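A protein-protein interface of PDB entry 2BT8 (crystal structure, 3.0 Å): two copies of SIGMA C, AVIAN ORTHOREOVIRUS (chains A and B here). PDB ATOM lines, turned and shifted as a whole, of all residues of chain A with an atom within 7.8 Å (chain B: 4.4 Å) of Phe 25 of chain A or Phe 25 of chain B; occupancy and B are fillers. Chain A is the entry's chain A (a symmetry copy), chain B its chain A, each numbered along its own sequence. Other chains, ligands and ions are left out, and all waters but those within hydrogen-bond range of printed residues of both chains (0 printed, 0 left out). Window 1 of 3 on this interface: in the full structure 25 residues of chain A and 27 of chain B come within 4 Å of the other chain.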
ATOM      1  N   MET A  21      34.941 -17.911  20.476  1.00  0.00           N
ATOM      2  CA  MET A  21      33.758 -17.124  20.795  1.00  0.00           C
ATOM      3  C   MET A  21      32.645 -17.235  19.742  1.00  0.00           C
ATOM      4  O   MET A  21      32.909 -17.183  18.557  1.00  0.00           O
ATOM      5  CB  MET A  21      34.169 -15.685  21.055  1.00  0.00           C
ATOM      6  CG  MET A  21      35.079 -15.572  22.257  1.00  0.00           C
ATOM      7  SD  MET A  21      35.760 -13.930  22.612  1.00  0.00           S
ATOM      8  CE  MET A  21      36.350 -13.397  20.978  1.00  0.00           C
ATOM      9  N   ASP A  22      31.407 -17.431  20.180  1.00  0.00           N
ATOM     10  CA  ASP A  22      30.260 -17.375  19.277  1.00  0.00           C
ATOM     11  C   ASP A  22      29.932 -15.904  19.022  1.00  0.00           C
ATOM     12  O   ASP A  22      29.491 -15.210  19.936  1.00  0.00           O
ATOM     13  CB  ASP A  22      29.056 -18.093  19.901  1.00  0.00           C
ATOM     14  CG  ASP A  22      27.749 -17.787  19.175  1.00  0.00           C
ATOM     15  OD1 ASP A  22      27.791 -17.234  18.051  1.00  0.00           O
ATOM     16  OD2 ASP A  22      26.674 -18.116  19.724  1.00  0.00           O
ATOM     17  N   PRO A  23      30.144 -15.422  17.788  1.00  0.00           N
ATOM     18  CA  PRO A  23      30.045 -13.972  17.573  1.00  0.00           C
ATOM     19  C   PRO A  23      28.626 -13.434  17.815  1.00  0.00           C
ATOM     20  O   PRO A  23      28.472 -12.241  18.149  1.00  0.00           O
ATOM     21  CB  PRO A  23      30.475 -13.776  16.101  1.00  0.00           C
ATOM     22  CG  PRO A  23      30.410 -15.116  15.477  1.00  0.00           C
ATOM     23  CD  PRO A  23      30.450 -16.163  16.554  1.00  0.00           C
ATOM     24  N   TYR A  24      27.620 -14.305  17.644  1.00  0.00           N
ATOM     25  CA  TYR A  24      26.248 -13.990  18.028  1.00  0.00           C
ATOM     26  C   TYR A  24      26.043 -13.914  19.524  1.00  0.00           C
ATOM     27  O   TYR A  24      24.981 -13.506  19.954  1.00  0.00           O
ATOM     28  CB  TYR A  24      25.253 -14.989  17.456  1.00  0.00           C
ATOM     29  CG  TYR A  24      25.168 -14.914  15.962  1.00  0.00           C
ATOM     30  CD1 TYR A  24      24.455 -13.882  15.331  1.00  0.00           C
ATOM     31  CD2 TYR A  24      25.822 -15.857  15.163  1.00  0.00           C
ATOM     32  CE1 TYR A  24      24.394 -13.799  13.934  1.00  0.00           C
ATOM     33  CE2 TYR A  24      25.757 -15.789  13.778  1.00  0.00           C
ATOM     34  CZ  TYR A  24      25.046 -14.763  13.173  1.00  0.00           C
ATOM     35  OH  TYR A  24      24.997 -14.706  11.807  1.00  0.00           O
ATOM     36  N   PHE A  25      27.034 -14.303  20.323  1.00  0.00           N
ATOM     37  CA  PHE A  25      26.866 -14.294  21.762  1.00  0.00           C
ATOM     38  C   PHE A  25      27.860 -13.466  22.537  1.00  0.00           C
ATOM     39  O   PHE A  25      27.551 -13.007  23.633  1.00  0.00           O
ATOM     40  CB  PHE A  25      26.854 -15.684  22.334  1.00  0.00           C
ATOM     41  CG  PHE A  25      26.781 -15.692  23.818  1.00  0.00           C
ATOM     42  CD1 PHE A  25      25.611 -15.332  24.466  1.00  0.00           C
ATOM     43  CD2 PHE A  25      27.904 -16.007  24.589  1.00  0.00           C
ATOM     44  CE1 PHE A  25      25.539 -15.310  25.860  1.00  0.00           C
ATOM     45  CE2 PHE A  25      27.844 -15.993  25.992  1.00  0.00           C
ATOM     46  CZ  PHE A  25      26.655 -15.648  26.629  1.00  0.00           C
ATOM     47  N   CYS A  26      29.061 -13.295  22.022  1.00  0.00           N
ATOM     48  CA  CYS A  26      30.085 -12.529  22.751  1.00  0.00           C
ATOM     49  C   CYS A  26      31.250 -12.278  21.852  1.00  0.00           C
ATOM     50  O   CYS A  26      31.308 -12.768  20.711  1.00  0.00           O
ATOM     51  CB  CYS A  26      30.583 -13.271  23.997  1.00  0.00           C
ATOM     52  SG  CYS A  26      31.344 -14.870  23.641  1.00  0.00           S
ATOM     53  N   SER A  27      32.193 -11.522  22.375  1.00  0.00           N
ATOM     54  CA  SER A  27      33.277 -11.047  21.575  1.00  0.00           C
ATOM     55  C   SER A  27      34.221 -10.360  22.538  1.00  0.00           C
ATOM     56  O   SER A  27      33.868 -10.158  23.709  1.00  0.00           O
ATOM     57  CB  SER A  27      32.731 -10.068  20.536  1.00  0.00           C
ATOM     58  OG  SER A  27      32.462  -8.797  21.104  1.00  0.00           O
ATOM     59  N   SER A  31      38.392  -7.118  26.927  1.00  0.00           N
ATOM     60  CA  SER A  31      37.686  -8.132  27.718  1.00  0.00           C
ATOM     61  C   SER A  31      36.505  -8.809  27.009  1.00  0.00           C
ATOM     62  O   SER A  31      36.105  -8.446  25.886  1.00  0.00           O
ATOM     63  CB  SER A  31      37.280  -7.595  29.086  1.00  0.00           C
ATOM     64  OG  SER A  31      36.131  -6.774  29.018  1.00  0.00           O
ATOM     65  N   LEU A  32      35.984  -9.832  27.673  1.00  0.00           N
ATOM     66  CA  LEU A  32      34.806 -10.556  27.222  1.00  0.00           C
ATOM     67  C   LEU A  32      33.572  -9.677  27.402  1.00  0.00           C
ATOM     68  O   LEU A  32      33.208  -9.316  28.527  1.00  0.00           O
ATOM     69  CB  LEU A  32      34.641 -11.833  28.046  1.00  0.00           C
ATOM     70  CG  LEU A  32      33.633 -12.787  27.441  1.00  0.00           C
ATOM     71  CD1 LEU A  32      33.966 -13.033  25.968  1.00  0.00           C
ATOM     72  CD2 LEU A  32      33.535 -14.090  28.235  1.00  0.00           C
ATOM     73  N   THR A  33      32.942  -9.340  26.284  1.00  0.00           N
ATOM     74  CA  THR A  33      31.764  -8.491  26.261  1.00  0.00           C
ATOM     75  C   THR A  33      30.662  -9.197  25.455  1.00  0.00           C
ATOM     76  O   THR A  33      30.777 -10.391  25.175  1.00  0.00           O
ATOM     77  CB  THR A  33      32.128  -7.129  25.678  1.00  0.00           C
ATOM     78  OG1 THR A  33      31.055  -6.201  25.905  1.00  0.00           O
ATOM     79  CG2 THR A  33      32.463  -7.240  24.167  1.00  0.00           C
ATOM     80  N   SER A  34      29.591  -8.499  25.086  1.00  0.00           N
ATOM     81  CA  SER A  34      28.490  -9.157  24.362  1.00  0.00           C
ATOM     82  C   SER A  34      28.720  -9.207  22.863  1.00  0.00           C
ATOM     83  O   SER A  34      29.701  -8.698  22.382  1.00  0.00           O
ATOM     84  CB  SER A  34      27.173  -8.473  24.661  1.00  0.00           C
ATOM     85  OG  SER A  34      27.372  -7.088  24.553  1.00  0.00           O
ATOM     86  N   TYR A  35      27.780  -9.802  22.142  1.00  0.00           N
ATOM     87  CA  TYR A  35      27.915 -10.128  20.721  1.00  0.00           C
ATOM     88  C   TYR A  35      28.468  -9.035  19.764  1.00  0.00           C
ATOM     89  O   TYR A  35      28.248  -7.831  19.948  1.00  0.00           O
ATOM     90  CB  TYR A  35      26.563 -10.663  20.205  1.00  0.00           C
ATOM     91  CG  TYR A  35      25.494  -9.602  19.925  1.00  0.00           C
ATOM     92  CD1 TYR A  35      24.685  -9.117  20.942  1.00  0.00           C
ATOM     93  CD2 TYR A  35      25.307  -9.087  18.634  1.00  0.00           C
ATOM     94  CE1 TYR A  35      23.714  -8.154  20.689  1.00  0.00           C
ATOM     95  CE2 TYR A  35      24.337  -8.119  18.370  1.00  0.00           C
ATOM     96  CZ  TYR A  35      23.544  -7.666  19.411  1.00  0.00           C
ATOM     97  OH  TYR A  35      22.588  -6.715  19.179  1.00  0.00           O
ATOM     98  N   SER A  36      29.145  -9.482  18.713  1.00  0.00           N
ATOM     99  CA  SER A  36      29.708  -8.581  17.718  1.00  0.00           C
ATOM    100  C   SER A  36      29.050  -8.765  16.368  1.00  0.00           C
ATOM    101  O   SER A  36      29.247  -7.939  15.479  1.00  0.00           O
ATOM    102  CB  SER A  36      31.200  -8.828  17.562  1.00  0.00           C
ATOM    103  OG  SER A  36      31.415 -10.178  17.171  1.00  0.00           O
ATOM    104  N   ALA A  37      28.292  -9.847  16.201  1.00  0.00           N
ATOM    105  CA  ALA A  37      27.584 -10.097  14.936  1.00  0.00           C
ATOM    106  C   ALA A  37      26.475  -9.088  14.666  1.00  0.00           C
ATOM    107  O   ALA A  37      25.672  -8.779  15.548  1.00  0.00           O
ATOM    108  CB  ALA A  37      27.006 -11.470  14.947  1.00  0.00           C
ATOM    109  N   GLY A  68      21.814 -10.447  18.433  1.00  0.00           N
ATOM    110  CA  GLY A  68      22.551 -11.343  19.316  1.00  0.00           C
ATOM    111  C   GLY A  68      21.907 -12.695  19.151  1.00  0.00           C
ATOM    112  O   GLY A  68      21.566 -13.087  18.052  1.00  0.00           O
ATOM    113  N   ARG A  69      21.713 -13.402  20.239  1.00  0.00           N
ATOM    114  CA  ARG A  69      21.033 -14.681  20.184  1.00  0.00           C
ATOM    115  C   ARG A  69      19.593 -14.541  20.696  1.00  0.00           C
ATOM    116  O   ARG A  69      19.012 -15.509  21.195  1.00  0.00           O
ATOM    117  CB  ARG A  69      21.789 -15.700  21.055  1.00  0.00           C
ATOM    118  CG  ARG A  69      23.119 -16.130  20.505  1.00  0.00           C
ATOM    119  CD  ARG A  69      23.347 -17.604  20.755  1.00  0.00           C
ATOM    120  NE  ARG A  69      22.754 -18.448  19.720  1.00  0.00           N
ATOM    121  CZ  ARG A  69      23.336 -18.769  18.562  1.00  0.00           C
ATOM    122  NH1 ARG A  69      24.553 -18.321  18.240  1.00  0.00           N
ATOM    123  NH2 ARG A  69      22.678 -19.539  17.709  1.00  0.00           N
ATOM    124  N   THR A 170      17.755 -18.039  20.853  1.00  0.00           N
ATOM    125  CA  THR A 170      18.299 -18.963  19.848  1.00  0.00           C
ATOM    126  C   THR A 170      19.656 -19.534  20.290  1.00  0.00           C
ATOM    127  O   THR A 170      20.287 -19.018  21.245  1.00  0.00           O
ATOM    128  CB  THR A 170      18.451 -18.308  18.456  1.00  0.00           C
ATOM    129  OG1 THR A 170      19.362 -17.199  18.527  1.00  0.00           O
ATOM    130  CG2 THR A 170      17.107 -17.834  17.952  1.00  0.00           C
ATOM    131  OXT THR A 170      20.132 -20.529  19.697  1.00  0.00           O
ATOM    132  N   ASP B  22      34.028  -7.995  30.974  1.00  0.00           N
ATOM    133  CA  ASP B  22      33.265  -6.751  30.934  1.00  0.00           C
ATOM    134  C   ASP B  22      32.179  -6.830  32.008  1.00  0.00           C
ATOM    135  O   ASP B  22      31.253  -7.627  31.882  1.00  0.00           O
ATOM    136  CB  ASP B  22      32.634  -6.557  29.548  1.00  0.00           C
ATOM    137  CG  ASP B  22      31.563  -5.471  29.536  1.00  0.00           C
ATOM    138  OD1 ASP B  22      31.474  -4.691  30.514  1.00  0.00           O
ATOM    139  OD2 ASP B  22      30.817  -5.384  28.536  1.00  0.00           O
ATOM    140  N   PRO B  23      32.285  -6.007  33.063  1.00  0.00           N
ATOM    141  CA  PRO B  23      31.385  -6.212  34.207  1.00  0.00           C
ATOM    142  C   PRO B  23      29.910  -5.973  33.847  1.00  0.00           C
ATOM    143  O   PRO B  23      29.018  -6.547  34.506  1.00  0.00           O
ATOM    144  CB  PRO B  23      31.875  -5.195  35.264  1.00  0.00           C
ATOM    145  CG  PRO B  23      32.737  -4.238  34.536  1.00  0.00           C
ATOM    146  CD  PRO B  23      33.193  -4.864  33.248  1.00  0.00           C
ATOM    147  N   TYR B  24      29.672  -5.140  32.823  1.00  0.00           N
ATOM    148  CA  TYR B  24      28.341  -4.977  32.249  1.00  0.00           C
ATOM    149  C   TYR B  24      27.860  -6.189  31.486  1.00  0.00           C
ATOM    150  O   TYR B  24      26.707  -6.224  31.100  1.00  0.00           O
ATOM    151  CB  TYR B  24      28.262  -3.767  31.329  1.00  0.00           C
ATOM    152  CG  TYR B  24      28.426  -2.477  32.072  1.00  0.00           C
ATOM    153  CD1 TYR B  24      27.370  -1.939  32.827  1.00  0.00           C
ATOM    154  CD2 TYR B  24      29.646  -1.793  32.052  1.00  0.00           C
ATOM    155  CE1 TYR B  24      27.529  -0.744  33.540  1.00  0.00           C
ATOM    156  CE2 TYR B  24      29.809  -0.601  32.747  1.00  0.00           C
ATOM    157  CZ  TYR B  24      28.753  -0.086  33.485  1.00  0.00           C
ATOM    158  OH  TYR B  24      28.932   1.084  34.169  1.00  0.00           O
ATOM    159  N   PHE B  25      28.720  -7.180  31.257  1.00  0.00           N
ATOM    160  CA  PHE B  25      28.318  -8.341  30.489  1.00  0.00           C
ATOM    161  C   PHE B  25      28.461  -9.672  31.181  1.00  0.00           C
ATOM    162  O   PHE B  25      27.745 -10.613  30.852  1.00  0.00           O
ATOM    163  CB  PHE B  25      29.031  -8.412  29.166  1.00  0.00           C
ATOM    164  CG  PHE B  25      28.706  -9.646  28.407  1.00  0.00           C
ATOM    165  CD1 PHE B  25      27.456  -9.808  27.830  1.00  0.00           C
ATOM    166  CD2 PHE B  25      29.630 -10.691  28.306  1.00  0.00           C
ATOM    167  CE1 PHE B  25      27.131 -10.975  27.137  1.00  0.00           C
ATOM    168  CE2 PHE B  25      29.317 -11.868  27.608  1.00  0.00           C
ATOM    169  CZ  PHE B  25      28.064 -12.007  27.017  1.00  0.00           C
ATOM    170  N   CYS B  26      29.394  -9.796  32.104  1.00  0.00           N
ATOM    171  CA  CYS B  26      29.605 -11.081  32.787  1.00  0.00           C
ATOM    172  C   CYS B  26      30.533 -10.885  33.941  1.00  0.00           C
ATOM    173  O   CYS B  26      31.080  -9.789  34.154  1.00  0.00           O
ATOM    174  CB  CYS B  26      30.207 -12.139  31.853  1.00  0.00           C
ATOM    175  SG  CYS B  26      31.819 -11.685  31.178  1.00  0.00           S
ATOM    176  N   SER B  34      26.392 -14.063  34.440  1.00  0.00           N
ATOM    177  CA  SER B  34      26.055 -12.779  33.800  1.00  0.00           C
ATOM    178  C   SER B  34      26.540 -11.581  34.595  1.00  0.00           C
ATOM    179  O   SER B  34      27.094 -11.740  35.654  1.00  0.00           O
ATOM    180  CB  SER B  34      24.562 -12.676  33.568  1.00  0.00           C
ATOM    181  OG  SER B  34      23.915 -13.079  34.746  1.00  0.00           O
ATOM    182  N   TYR B  35      26.292 -10.388  34.075  1.00  0.00           N
ATOM    183  CA  TYR B  35      26.852  -9.135  34.582  1.00  0.00           C
ATOM    184  C   TYR B  35      26.811  -8.876  36.114  1.00  0.00           C
ATOM    185  O   TYR B  35      25.889  -9.297  36.825  1.00  0.00           O
ATOM    186  CB  TYR B  35      26.208  -7.958  33.820  1.00  0.00           C
ATOM    187  CG  TYR B  35      24.792  -7.578  34.264  1.00  0.00           C
ATOM    188  CD1 TYR B  35      23.683  -8.246  33.765  1.00  0.00           C
ATOM    189  CD2 TYR B  35      24.577  -6.548  35.191  1.00  0.00           C
ATOM    190  CE1 TYR B  35      22.397  -7.901  34.166  1.00  0.00           C
ATOM    191  CE2 TYR B  35      23.290  -6.196  35.603  1.00  0.00           C
ATOM    192  CZ  TYR B  35      22.209  -6.881  35.075  1.00  0.00           C
ATOM    193  OH  TYR B  35      20.938  -6.557  35.464  1.00  0.00           O
ATOM    194  N   ARG B  69      24.036  -5.107  29.556  1.00  0.00           N
ATOM    195  CA  ARG B  69      24.275  -4.390  28.320  1.00  0.00           C
ATOM    196  C   ARG B  69      22.971  -4.255  27.522  1.00  0.00           C
ATOM    197  O   ARG B  69      23.000  -4.146  26.292  1.00  0.00           O
ATOM    198  CB  ARG B  69      25.312  -5.154  27.478  1.00  0.00           C
ATOM    199  CG  ARG B  69      26.710  -5.123  28.028  1.00  0.00           C
ATOM    200  CD  ARG B  69      27.719  -4.998  26.909  1.00  0.00           C
ATOM    201  NE  ARG B  69      27.948  -3.610  26.512  1.00  0.00           N
ATOM    202  CZ  ARG B  69      28.807  -2.774  27.099  1.00  0.00           C
ATOM    203  NH1 ARG B  69      29.552  -3.150  28.142  1.00  0.00           N
ATOM    204  NH2 ARG B  69      28.907  -1.536  26.639  1.00  0.00           N
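Among the printed residues, merely in contact across the chains: Phe 25 of chain A with Phe 25 of chain B, Leu 32 of chain A with Phe 25 of chain B, Leu 32 of chain A with Cys 26 of chain B, Thr 33 of chain A with Phe 25 of chain B, Thr 33 of chain A with Arg 69 of chain B, Ser 34 of chain A with Phe 25 of chain B and Ser 34 of chain A with Arg 69 of chain B.
The backbone NH (N) of Tyr 24 of chain B sits at hydrogen-bond distance from the side-chain carboxylate (OD1) of Asp 22 of chain B. OD2 of Asp 22 of chain B is in salt-bridge range of NH1 of Arg 69 of chain B (2.6 Å). The backbone NH (N) of Arg 69 of chain B lies close to the backbone carbonyl oxygen (O) of Tyr 24 of chain B (3.3 Å). The backbone carbonyl oxygen (O) of Ser 27 of chain A lies within hydrogen-bond range of the backbone NH (N) of Thr 33 of chain A, 2.9 Å away. O of Ser 34 of chain A lies within hydrogen-bond range of OG of Ser 27 of chain A (3.0 Å).
Phe 25 of chain B touches its own counterpart, Phe 25 of chain A. Ser 34 of chain A touches Phe 25 of chain B, but with the chains exchanged Phe 25 of chain A does not touch Ser 34 of chain B (7.7 Å). Ser 34 of chain A touches Arg 69 of chain B, but with the chains exchanged Arg 69 of chain A does not touch Ser 34 of chain B (13.2 Å).
Phe 25 of chain A touches just one residue of chain B: Phe 25 (3.6 Å). Printed residues of chain A within 4 Å of Phe 25 of chain B: Phe 25, Leu 32, Thr 33 and Ser 34. Printed residues of chain B within 4 Å of Ser 34 of chain A: Phe 25 (3.5 Å) and Arg 69 (3.2 Å). Of the printed residues of chain B, Ser 31 of chain A touches Asp 22. Of the printed residues of chain A, Asp 22 of chain B touches Ser 31, Leu 32 and Thr 33. Printed residues of chain A within 4 Å of Arg 69 of chain B: Thr 33 (3.7 Å) and Ser 34 (3.2 Å). Of the printed residues of chain A, Cys 26 of chain B touches Leu 32 (3.8 Å). The nearest printed residue of chain B that does not touch Phe 25 of chain A is Cys 26 of chain B (7.2 Å). The nearest printed residue of chain B that does not touch Ser 31 of chain A is Pro 23 of chain B (5.5 Å).
Hydrophobic or aromatic side chains of chain B within 4 Å of the printed part of chain A: Phe 25. Among the printed residues, 10 pairs touch across the chains. Among the printed residues, no Asp or Glu carboxylate lies within 4 Å of a Lys or Arg side-chain nitrogen of the other chain.
The side-chain hydroxyl (OG) of Ser 31 of chain A sits at hydrogen-bond distance from the backbone NH (N) of Asp 22 of chain B, 3.1 Å away. The backbone NH (N) of Asp 22 of chain B lies within hydrogen-bond range of the backbone carbonyl oxygen (O) of Leu 32 of chain A, at 2.9 Å. The side-chain hydroxyl of Thr 33 of chain A lies within hydrogen-bond range of the side-chain carboxylate of Asp 22 of chain B, 2.8 Å away.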
